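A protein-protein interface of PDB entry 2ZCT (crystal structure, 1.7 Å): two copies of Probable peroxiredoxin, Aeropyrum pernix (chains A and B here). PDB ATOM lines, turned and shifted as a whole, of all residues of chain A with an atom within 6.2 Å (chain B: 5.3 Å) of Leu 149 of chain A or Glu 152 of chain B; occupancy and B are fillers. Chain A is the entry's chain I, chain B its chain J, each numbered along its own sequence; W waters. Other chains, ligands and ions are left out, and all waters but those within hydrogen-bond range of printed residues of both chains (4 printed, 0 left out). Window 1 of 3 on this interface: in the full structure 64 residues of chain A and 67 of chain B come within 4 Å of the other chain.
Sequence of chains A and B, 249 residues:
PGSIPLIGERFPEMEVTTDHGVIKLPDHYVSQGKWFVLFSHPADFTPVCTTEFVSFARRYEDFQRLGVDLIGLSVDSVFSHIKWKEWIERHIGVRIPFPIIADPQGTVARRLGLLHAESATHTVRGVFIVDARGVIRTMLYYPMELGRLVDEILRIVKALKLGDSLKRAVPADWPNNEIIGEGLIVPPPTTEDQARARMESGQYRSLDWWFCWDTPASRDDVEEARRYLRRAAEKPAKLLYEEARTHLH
Tyr 142 of chain A touches Glu 152 of chain B, and with the chains exchanged Glu 152 of chain A touches Tyr 142 of chain B.
Leu 149 of chain A touches Glu 152 of chain B, and with the chains exchanged Glu 152 of chain A touches Leu 149 of chain B.
Leu 149 of chain A touches Leu 229 of chain B, and with the chains exchanged Leu 229 of chain A touches Leu 149 of chain B.
8 positions are printed for both chains.
Of the 16 pairs that touch across the chains among the printed residues, 6 have their exchanged pair printed and touching as well.
Hydrophobic or aromatic side chains of chain A within 4 Å of the printed part of chain B: Tyr 142, Leu 146, Leu 149, Val 150 and Leu 229.
Among the printed residues, 16 pairs touch across the chains.
Among the printed residues, no Asp or Glu carboxylate lies within 4 Å of a Lys or Arg side-chain nitrogen of the other chain.
Water W2 bridges the backbone carbonyl oxygen of Ala 232 of chain A (2.6 Å) and the backbone carbonyl oxygen of Asp 173 of chain B (3.0 Å).
Water W3 lies within hydrogen-bond range of OD1 of Asp 173 of chain B, OD2 of Asp 151 of chain A and N of Val 150 of chain A.
Water W1 bridges the backbone carbonyl oxygen of Gly 147 of chain A and the guanidinium group of Arg 155 of chain B.
Water W4 bridges the backbone carbonyl oxygen of Leu 229 of chain A (2.9 Å) and the backbone carbonyl oxygen of Leu 229 of chain B (2.9 Å).
N of Asp 173 of chain B lies within hydrogen-bond range of O of Arg 148 of chain A (3.0 Å).
O of Gly 147 of chain A is in hydrogen-bond range of NH2 of Arg 155 of chain B, at 3.3 Å.
The side-chain carboxylate (OE2) of Glu 152 of chain B is in hydrogen-bond range of the side-chain hydroxyl (OH) of Tyr 142 of chain A, 2.5 Å away.
OE2 of Glu 152 of chain A is in hydrogen-bond range of OH of Tyr 142 of chain B, at 2.5 Å.
OG of Ser 55 of chain A is in hydrogen-bond range of OD2 of Asp 173 of chain B.
The side-chain carboxylate (OD1) of Asp 173 of chain B sits at hydrogen-bond distance from the backbone NH (N) of Val 150 of chain A, at 2.9 Å.
The side-chain carboxylate of Asp 151 of chain A is in hydrogen-bond range of the backbone NH of Ala 232 of chain A (3.4 Å).
The guanidinium group of Arg 155 of chain B is in salt-bridge range of the side-chain carboxylate of Glu 152 of chain B, 2.6 Å away.
The side-chain carboxylate (OE1) of Glu 52 of chain A is in salt-bridge range of the guanidinium group (NH2) of Arg 148 of chain A, at 3.1 Å.
Among the printed residues, pairs that only touch across the chains: Tyr 142 of chain A with Arg 155 of chain B (3.98 Å), Tyr 142 of chain A with Ile 156 of chain B (3.7 Å), Leu 146 of chain A with Ile 156 of chain B (3.6 Å), Leu 149 of chain A with Glu 152 of chain B (3.5 Å), Leu 149 of chain A with Arg 155 of chain B (3.9 Å), Leu 149 of chain A with Asp 173 of chain B (3.6 Å), Leu 149 of chain A with Leu 229 of chain B (3.8 Å), Glu 152 of chain A with Leu 149 of chain B (3.4 Å), Leu 229 of chain A with Leu 149 of chain B (3.9 Å) and Ala 232 of chain A with Leu 229 of chain B (3.5 Å).
Of chain B, only Glu 152, Arg 155, Asp 173 and Leu 229 come within 4 Å of Leu 149 of chain A.
Of the printed residues of chain A, Glu 152 of chain B touches Tyr 142 and Leu 149.
Of the printed residues of chain A, Arg 155 of chain B touches Tyr 142 (3.98 Å), Gly 147 (3.3 Å) and Leu 149 (3.9 Å).
Printed residues of chain A within 4 Å of Asp 173 of chain B: Ser 55 (2.7 Å), Arg 148 (3.0 Å), Leu 149 (3.6 Å) and Val 150 (2.9 Å).
Printed residues of chain A within 4 Å of Tyr 142 of chain B: Glu 152.
Printed residues of chain B within 4 Å of Arg 148 of chain A: Asp 173 (3.0 Å).
Of the printed residues of chain B, Leu 229 of chain A touches Leu 149 (3.9 Å).
Val 157 of chain B touches none of the printed residues of chain A.
Asp 151 of chain A touches none of the printed residues of chain B.
The nearest printed residue of chain B that does not touch Tyr 142 of chain A is Tyr 142 of chain B (5.4 Å).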
ATOM      1  N   GLU A  52      31.765 -13.481  -7.107  1.00  0.00           N
ATOM      2  CA  GLU A  52      30.438 -13.558  -6.503  1.00  0.00           C
ATOM      3  C   GLU A  52      29.415 -12.728  -7.252  1.00  0.00           C
ATOM      4  O   GLU A  52      28.275 -13.161  -7.460  1.00  0.00           O
ATOM      5  CB  GLU A  52      30.521 -13.150  -5.018  1.00  0.00           C
ATOM      6  CG  GLU A  52      31.245 -14.215  -4.214  1.00  0.00           C
ATOM      7  CD  GLU A  52      31.615 -13.743  -2.817  1.00  0.00           C
ATOM      8  OE1 GLU A  52      31.811 -12.526  -2.626  1.00  0.00           O
ATOM      9  OE2 GLU A  52      31.654 -14.574  -1.913  1.00  0.00           O
ATOM     10  N   SER A  55      28.381 -14.744 -10.274  1.00  0.00           N
ATOM     11  CA  SER A  55      27.529 -15.866  -9.904  1.00  0.00           C
ATOM     12  C   SER A  55      26.106 -15.408  -9.605  1.00  0.00           C
ATOM     13  O   SER A  55      25.131 -16.004 -10.094  1.00  0.00           O
ATOM     14  CB  SER A  55      28.132 -16.578  -8.691  1.00  0.00           C
ATOM     15  OG  SER A  55      27.312 -17.665  -8.350  1.00  0.00           O
ATOM     16  N   TYR A 142      30.770 -15.573   5.284  1.00  0.00           N
ATOM     17  CA  TYR A 142      31.949 -16.124   4.612  1.00  0.00           C
ATOM     18  C   TYR A 142      33.011 -15.047   4.554  1.00  0.00           C
ATOM     19  O   TYR A 142      32.688 -13.911   4.120  1.00  0.00           O
ATOM     20  CB  TYR A 142      31.591 -16.478   3.162  1.00  0.00           C
ATOM     21  CG  TYR A 142      30.730 -17.720   3.001  1.00  0.00           C
ATOM     22  CD1 TYR A 142      29.386 -17.723   3.372  1.00  0.00           C
ATOM     23  CD2 TYR A 142      31.252 -18.865   2.435  1.00  0.00           C
ATOM     24  CE1 TYR A 142      28.589 -18.855   3.189  1.00  0.00           C
ATOM     25  CE2 TYR A 142      30.481 -20.018   2.282  1.00  0.00           C
ATOM     26  CZ  TYR A 142      29.138 -19.997   2.649  1.00  0.00           C
ATOM     27  OH  TYR A 142      28.360 -21.125   2.465  1.00  0.00           O
ATOM     28  N   LEU A 146      37.086 -16.482   0.898  1.00  0.00           N
ATOM     29  CA  LEU A 146      36.289 -17.659   0.565  1.00  0.00           C
ATOM     30  C   LEU A 146      35.004 -17.197  -0.079  1.00  0.00           C
ATOM     31  O   LEU A 146      34.170 -16.622   0.584  1.00  0.00           O
ATOM     32  CB  LEU A 146      35.834 -18.398   1.816  1.00  0.00           C
ATOM     33  CG  LEU A 146      35.572 -19.907   1.869  1.00  0.00           C
ATOM     34  CD1 LEU A 146      34.496 -20.337   2.929  1.00  0.00           C
ATOM     35  CD2 LEU A 146      35.514 -20.709   0.539  1.00  0.00           C
ATOM     36  N   GLY A 147      34.842 -17.469  -1.370  1.00  0.00           N
ATOM     37  CA  GLY A 147      33.599 -17.131  -2.028  1.00  0.00           C
ATOM     38  C   GLY A 147      32.419 -17.927  -1.541  1.00  0.00           C
ATOM     39  O   GLY A 147      32.515 -19.123  -1.139  1.00  0.00           O
ATOM     40  N   ARG A 148      31.248 -17.294  -1.630  1.00  0.00           N
ATOM     41  CA  ARG A 148      30.012 -17.930  -1.253  1.00  0.00           C
ATOM     42  C   ARG A 148      29.616 -19.033  -2.238  1.00  0.00           C
ATOM     43  O   ARG A 148      30.148 -19.063  -3.351  1.00  0.00           O
ATOM     44  CB  ARG A 148      28.904 -16.868  -1.144  1.00  0.00           C
ATOM     45  CG  ARG A 148      29.212 -15.858  -0.039  1.00  0.00           C
ATOM     46  CD  ARG A 148      28.792 -14.461  -0.462  1.00  0.00           C
ATOM     47  NE  ARG A 148      29.093 -13.434   0.534  1.00  0.00           N
ATOM     48  CZ  ARG A 148      29.236 -12.149   0.216  1.00  0.00           C
ATOM     49  NH1 ARG A 148      29.462 -11.252   1.157  1.00  0.00           N
ATOM     50  NH2 ARG A 148      29.181 -11.781  -1.063  1.00  0.00           N
ATOM     51  N   LEU A 149      28.735 -19.935  -1.786  1.00  0.00           N
ATOM     52  CA  LEU A 149      28.022 -20.887  -2.643  1.00  0.00           C
ATOM     53  C   LEU A 149      26.613 -20.331  -2.977  1.00  0.00           C
ATOM     54  O   LEU A 149      25.658 -20.434  -2.201  1.00  0.00           O
ATOM     55  CB  LEU A 149      27.929 -22.279  -1.999  1.00  0.00           C
ATOM     56  CG  LEU A 149      27.411 -23.406  -2.912  1.00  0.00           C
ATOM     57  CD1 LEU A 149      28.465 -23.813  -3.934  1.00  0.00           C
ATOM     58  CD2 LEU A 149      27.014 -24.634  -2.049  1.00  0.00           C
ATOM     59  N   VAL A 150      26.504 -19.701  -4.159  1.00  0.00           N
ATOM     60  CA  VAL A 150      25.327 -18.889  -4.383  1.00  0.00           C
ATOM     61  C   VAL A 150      24.068 -19.761  -4.537  1.00  0.00           C
ATOM     62  O   VAL A 150      22.968 -19.336  -4.171  1.00  0.00           O
ATOM     63  CB  VAL A 150      25.527 -17.924  -5.584  1.00  0.00           C
ATOM     64  CG1 VAL A 150      24.237 -17.163  -5.906  1.00  0.00           C
ATOM     65  CG2 VAL A 150      26.625 -16.894  -5.287  1.00  0.00           C
ATOM     66  N   ASP A 151      24.202 -20.983  -5.070  1.00  0.00           N
ATOM     67  CA  ASP A 151      23.051 -21.902  -5.190  1.00  0.00           C
ATOM     68  C   ASP A 151      22.433 -22.289  -3.834  1.00  0.00           C
ATOM     69  O   ASP A 151      21.233 -22.566  -3.727  1.00  0.00           O
ATOM     70  CB  ASP A 151      23.460 -23.153  -5.973  1.00  0.00           C
ATOM     71  CG  ASP A 151      23.650 -22.865  -7.458  1.00  0.00           C
ATOM     72  OD1 ASP A 151      22.760 -22.239  -8.070  1.00  0.00           O
ATOM     73  OD2 ASP A 151      24.719 -23.219  -8.002  1.00  0.00           O
ATOM     74  N   GLU A 152      23.263 -22.260  -2.797  1.00  0.00           N
ATOM     75  CA  GLU A 152      22.797 -22.504  -1.417  1.00  0.00           C
ATOM     76  C   GLU A 152      21.928 -21.339  -0.937  1.00  0.00           C
ATOM     77  O   GLU A 152      20.977 -21.530  -0.163  1.00  0.00           O
ATOM     78  CB  GLU A 152      24.001 -22.744  -0.486  1.00  0.00           C
ATOM     79  CG  GLU A 152      23.635 -22.835   1.034  1.00  0.00           C
ATOM     80  CD  GLU A 152      22.537 -23.869   1.400  1.00  0.00           C
ATOM     81  OE1 GLU A 152      22.028 -24.605   0.523  1.00  0.00           O
ATOM     82  OE2 GLU A 152      22.159 -23.929   2.599  1.00  0.00           O
ATOM     83  N   ILE A 153      22.253 -20.119  -1.393  1.00  0.00           N
ATOM     84  CA  ILE A 153      21.441 -18.947  -1.050  1.00  0.00           C
ATOM     85  C   ILE A 153      20.043 -19.092  -1.689  1.00  0.00           C
ATOM     86  O   ILE A 153      19.056 -18.800  -1.065  1.00  0.00           O
ATOM     87  CB  ILE A 153      22.152 -17.605  -1.413  1.00  0.00           C
ATOM     88  CG1 ILE A 153      23.489 -17.499  -0.654  1.00  0.00           C
ATOM     89  CG2 ILE A 153      21.305 -16.430  -1.033  1.00  0.00           C
ATOM     90  CD1 ILE A 153      24.371 -16.266  -1.005  1.00  0.00           C
ATOM     91  N   LEU A 154      19.984 -19.597  -2.924  1.00  0.00           N
ATOM     92  CA  LEU A 154      18.697 -19.903  -3.578  1.00  0.00           C
ATOM     93  C   LEU A 154      17.958 -21.003  -2.812  1.00  0.00           C
ATOM     94  O   LEU A 154      16.743 -20.924  -2.602  1.00  0.00           O
ATOM     95  CB  LEU A 154      18.974 -20.335  -5.038  1.00  0.00           C
ATOM     96  CG  LEU A 154      19.207 -19.195  -6.007  1.00  0.00           C
ATOM     97  CD1 LEU A 154      19.827 -19.721  -7.295  1.00  0.00           C
ATOM     98  CD2 LEU A 154      17.874 -18.469  -6.286  1.00  0.00           C
ATOM     99  N   LEU A 229      21.030 -27.492  -6.069  1.00  0.00           N
ATOM    100  CA  LEU A 229      22.143 -28.327  -5.528  1.00  0.00           C
ATOM    101  C   LEU A 229      22.900 -29.053  -6.638  1.00  0.00           C
ATOM    102  O   LEU A 229      24.137 -29.093  -6.657  1.00  0.00           O
ATOM    103  CB  LEU A 229      21.608 -29.342  -4.514  1.00  0.00           C
ATOM    104  CG  LEU A 229      21.000 -28.714  -3.245  1.00  0.00           C
ATOM    105  CD1 LEU A 229      20.451 -29.827  -2.336  1.00  0.00           C
ATOM    106  CD2 LEU A 229      22.047 -27.814  -2.523  1.00  0.00           C
ATOM    107  N   ALA A 232      25.060 -26.544  -8.301  1.00  0.00           N
ATOM    108  CA  ALA A 232      26.260 -26.310  -7.442  1.00  0.00           C
ATOM    109  C   ALA A 232      27.323 -27.380  -7.637  1.00  0.00           C
ATOM    110  O   ALA A 232      28.534 -27.096  -7.628  1.00  0.00           O
ATOM    111  CB  ALA A 232      25.847 -26.275  -5.954  1.00  0.00           C
ATOM    112  N   TYR B 142      21.716 -20.009  10.192  1.00  0.00           N
ATOM    113  CA  TYR B 142      20.466 -20.551   9.666  1.00  0.00           C
ATOM    114  C   TYR B 142      19.474 -20.562  10.828  1.00  0.00           C
ATOM    115  O   TYR B 142      19.828 -20.994  11.945  1.00  0.00           O
ATOM    116  CB  TYR B 142      20.679 -22.002   9.218  1.00  0.00           C
ATOM    117  CG  TYR B 142      21.445 -22.197   7.932  1.00  0.00           C
ATOM    118  CD1 TYR B 142      22.823 -21.960   7.867  1.00  0.00           C
ATOM    119  CD2 TYR B 142      20.810 -22.687   6.787  1.00  0.00           C
ATOM    120  CE1 TYR B 142      23.533 -22.153   6.671  1.00  0.00           C
ATOM    121  CE2 TYR B 142      21.505 -22.881   5.597  1.00  0.00           C
ATOM    122  CZ  TYR B 142      22.868 -22.629   5.545  1.00  0.00           C
ATOM    123  OH  TYR B 142      23.568 -22.835   4.381  1.00  0.00           O
ATOM    124  N   LEU B 149      22.888 -26.993   5.482  1.00  0.00           N
ATOM    125  CA  LEU B 149      23.418 -27.862   4.431  1.00  0.00           C
ATOM    126  C   LEU B 149      24.791 -28.340   4.899  1.00  0.00           C
ATOM    127  O   LEU B 149      25.782 -27.635   4.731  1.00  0.00           O
ATOM    128  CB  LEU B 149      23.547 -27.101   3.108  1.00  0.00           C
ATOM    129  CG  LEU B 149      23.836 -28.014   1.915  1.00  0.00           C
ATOM    130  CD1 LEU B 149      22.657 -28.947   1.621  1.00  0.00           C
ATOM    131  CD2 LEU B 149      24.200 -27.169   0.665  1.00  0.00           C
ATOM    132  N   VAL B 150      24.861 -29.524   5.505  1.00  0.00           N
ATOM    133  CA  VAL B 150      26.142 -29.869   6.190  1.00  0.00           C
ATOM    134  C   VAL B 150      27.328 -30.065   5.258  1.00  0.00           C
ATOM    135  O   VAL B 150      28.472 -29.729   5.616  1.00  0.00           O
ATOM    136  CB  VAL B 150      26.000 -31.052   7.200  1.00  0.00           C
ATOM    137  CG1 VAL B 150      27.361 -31.341   7.924  1.00  0.00           C
ATOM    138  CG2 VAL B 150      24.969 -30.697   8.218  1.00  0.00           C
ATOM    139  N   ASP B 151      27.082 -30.579   4.051  1.00  0.00           N
ATOM    140  CA  ASP B 151      28.139 -30.687   3.044  1.00  0.00           C
ATOM    141  C   ASP B 151      28.789 -29.341   2.661  1.00  0.00           C
ATOM    142  O   ASP B 151      29.976 -29.309   2.355  1.00  0.00           O
ATOM    143  CB  ASP B 151      27.614 -31.394   1.812  1.00  0.00           C
ATOM    144  CG  ASP B 151      27.343 -32.842   2.068  1.00  0.00           C
ATOM    145  OD1 ASP B 151      28.260 -33.524   2.562  1.00  0.00           O
ATOM    146  OD2 ASP B 151      26.212 -33.290   1.793  1.00  0.00           O
ATOM    147  N   GLU B 152      28.045 -28.246   2.751  1.00  0.00           N
ATOM    148  CA  GLU B 152      28.608 -26.914   2.510  1.00  0.00           C
ATOM    149  C   GLU B 152      29.610 -26.545   3.627  1.00  0.00           C
ATOM    150  O   GLU B 152      30.627 -25.882   3.397  1.00  0.00           O
ATOM    151  CB  GLU B 152      27.488 -25.884   2.398  1.00  0.00           C
ATOM    152  CG  GLU B 152      27.942 -24.425   2.230  1.00  0.00           C
ATOM    153  CD  GLU B 152      29.060 -24.142   1.180  1.00  0.00           C
ATOM    154  OE1 GLU B 152      29.480 -25.008   0.372  1.00  0.00           O
ATOM    155  OE2 GLU B 152      29.544 -23.001   1.214  1.00  0.00           O
ATOM    156  N   ILE B 153      29.301 -26.984   4.836  1.00  0.00           N
ATOM    157  CA  ILE B 153      30.221 -26.769   5.948  1.00  0.00           C
ATOM    158  C   ILE B 153      31.518 -27.523   5.681  1.00  0.00           C
ATOM    159  O   ILE B 153      32.611 -27.017   5.935  1.00  0.00           O
ATOM    160  CB  ILE B 153      29.572 -27.182   7.289  1.00  0.00           C
ATOM    161  CG1 ILE B 153      28.322 -26.312   7.543  1.00  0.00           C
ATOM    162  CG2 ILE B 153      30.618 -27.098   8.409  1.00  0.00           C
ATOM    163  CD1 ILE B 153      27.580 -26.618   8.861  1.00  0.00           C
ATOM    164  N   LEU B 154      31.408 -28.743   5.131  1.00  0.00           N
ATOM    165  CA  LEU B 154      32.614 -29.475   4.725  1.00  0.00           C
ATOM    166  C   LEU B 154      33.373 -28.716   3.626  1.00  0.00           C
ATOM    167  O   LEU B 154      34.608 -28.587   3.666  1.00  0.00           O
ATOM    168  CB  LEU B 154      32.212 -30.882   4.268  1.00  0.00           C
ATOM    169  CG  LEU B 154      32.040 -31.883   5.424  1.00  0.00           C
ATOM    170  CD1 LEU B 154      31.449 -33.124   4.825  1.00  0.00           C
ATOM    171  CD2 LEU B 154      33.406 -32.193   6.081  1.00  0.00           C
ATOM    172  N   ARG B 155      32.643 -28.185   2.657  1.00  0.00           N
ATOM    173  CA  ARG B 155      33.297 -27.424   1.571  1.00  0.00           C
ATOM    174  C   ARG B 155      34.027 -26.188   2.107  1.00  0.00           C
ATOM    175  O   ARG B 155      35.154 -25.923   1.702  1.00  0.00           O
ATOM    176  CB  ARG B 155      32.297 -27.022   0.488  1.00  0.00           C
ATOM    177  CG  ARG B 155      32.934 -26.567  -0.843  1.00  0.00           C
ATOM    178  CD  ARG B 155      31.909 -25.830  -1.739  1.00  0.00           C
ATOM    179  NE  ARG B 155      31.530 -24.547  -1.142  1.00  0.00           N
ATOM    180  CZ  ARG B 155      32.114 -23.379  -1.399  1.00  0.00           C
ATOM    181  NH1 ARG B 155      33.083 -23.282  -2.315  1.00  0.00           N
ATOM    182  NH2 ARG B 155      31.719 -22.293  -0.742  1.00  0.00           N
ATOM    183  N   ILE B 156      33.411 -25.497   3.066  1.00  0.00           N
ATOM    184  CA  ILE B 156      33.971 -24.296   3.671  1.00  0.00           C
ATOM    185  C   ILE B 156      35.302 -24.662   4.335  1.00  0.00           C
ATOM    186  O   ILE B 156      36.293 -24.036   4.083  1.00  0.00           O
ATOM    187  CB  ILE B 156      33.011 -23.681   4.679  1.00  0.00           C
ATOM    188  CG1 ILE B 156      31.838 -22.990   3.931  1.00  0.00           C
ATOM    189  CG2 ILE B 156      33.705 -22.665   5.594  1.00  0.00           C
ATOM    190  CD1 ILE B 156      30.673 -22.699   4.865  1.00  0.00           C
ATOM    191  N   VAL B 157      35.308 -25.663   5.207  1.00  0.00           N
ATOM    192  CA  VAL B 157      36.560 -25.986   5.896  1.00  0.00           C
ATOM    193  C   VAL B 157      37.659 -26.426   4.952  1.00  0.00           C
ATOM    194  O   VAL B 157      38.801 -26.002   5.094  1.00  0.00           O
ATOM    195  CB  VAL B 157      36.372 -27.065   6.955  1.00  0.00           C
ATOM    196  CG1 VAL B 157      37.801 -27.418   7.506  1.00  0.00           C
ATOM    197  CG2 VAL B 157      35.497 -26.548   8.023  1.00  0.00           C
ATOM    198  N   ASP B 173      31.640 -20.441  -5.571  1.00  0.00           N
ATOM    199  CA  ASP B 173      31.173 -21.746  -6.101  1.00  0.00           C
ATOM    200  C   ASP B 173      32.285 -22.750  -6.386  1.00  0.00           C
ATOM    201  O   ASP B 173      32.062 -23.782  -7.064  1.00  0.00           O
ATOM    202  CB  ASP B 173      30.286 -21.573  -7.353  1.00  0.00           C
ATOM    203  CG  ASP B 173      29.238 -20.466  -7.206  1.00  0.00           C
ATOM    204  OD1 ASP B 173      28.458 -20.470  -6.214  1.00  0.00           O
ATOM    205  OD2 ASP B 173      29.180 -19.596  -8.113  1.00  0.00           O
ATOM    206  N   LEU B 229      29.613 -31.547  -2.582  1.00  0.00           N
ATOM    207  CA  LEU B 229      28.495 -30.980  -3.329  1.00  0.00           C
ATOM    208  C   LEU B 229      27.678 -32.049  -4.054  1.00  0.00           C
ATOM    209  O   LEU B 229      26.441 -32.005  -4.035  1.00  0.00           O
ATOM    210  CB  LEU B 229      28.998 -29.896  -4.298  1.00  0.00           C
ATOM    211  CG  LEU B 229      29.602 -28.683  -3.587  1.00  0.00           C
ATOM    212  CD1 LEU B 229      30.104 -27.670  -4.608  1.00  0.00           C
ATOM    213  CD2 LEU B 229      28.640 -28.043  -2.542  1.00  0.00           C
HETATM  214  O   HOH W   1      34.254 -20.749  -2.497  1.00  0.00           O
HETATM  215  O   HOH W   2      29.181 -24.603  -7.441  1.00  0.00           O
HETATM  216  O   HOH W   3      26.598 -22.347  -6.165  1.00  0.00           O
HETATM  217  O   HOH W   4      25.245 -29.367  -4.035  1.00  0.00           O
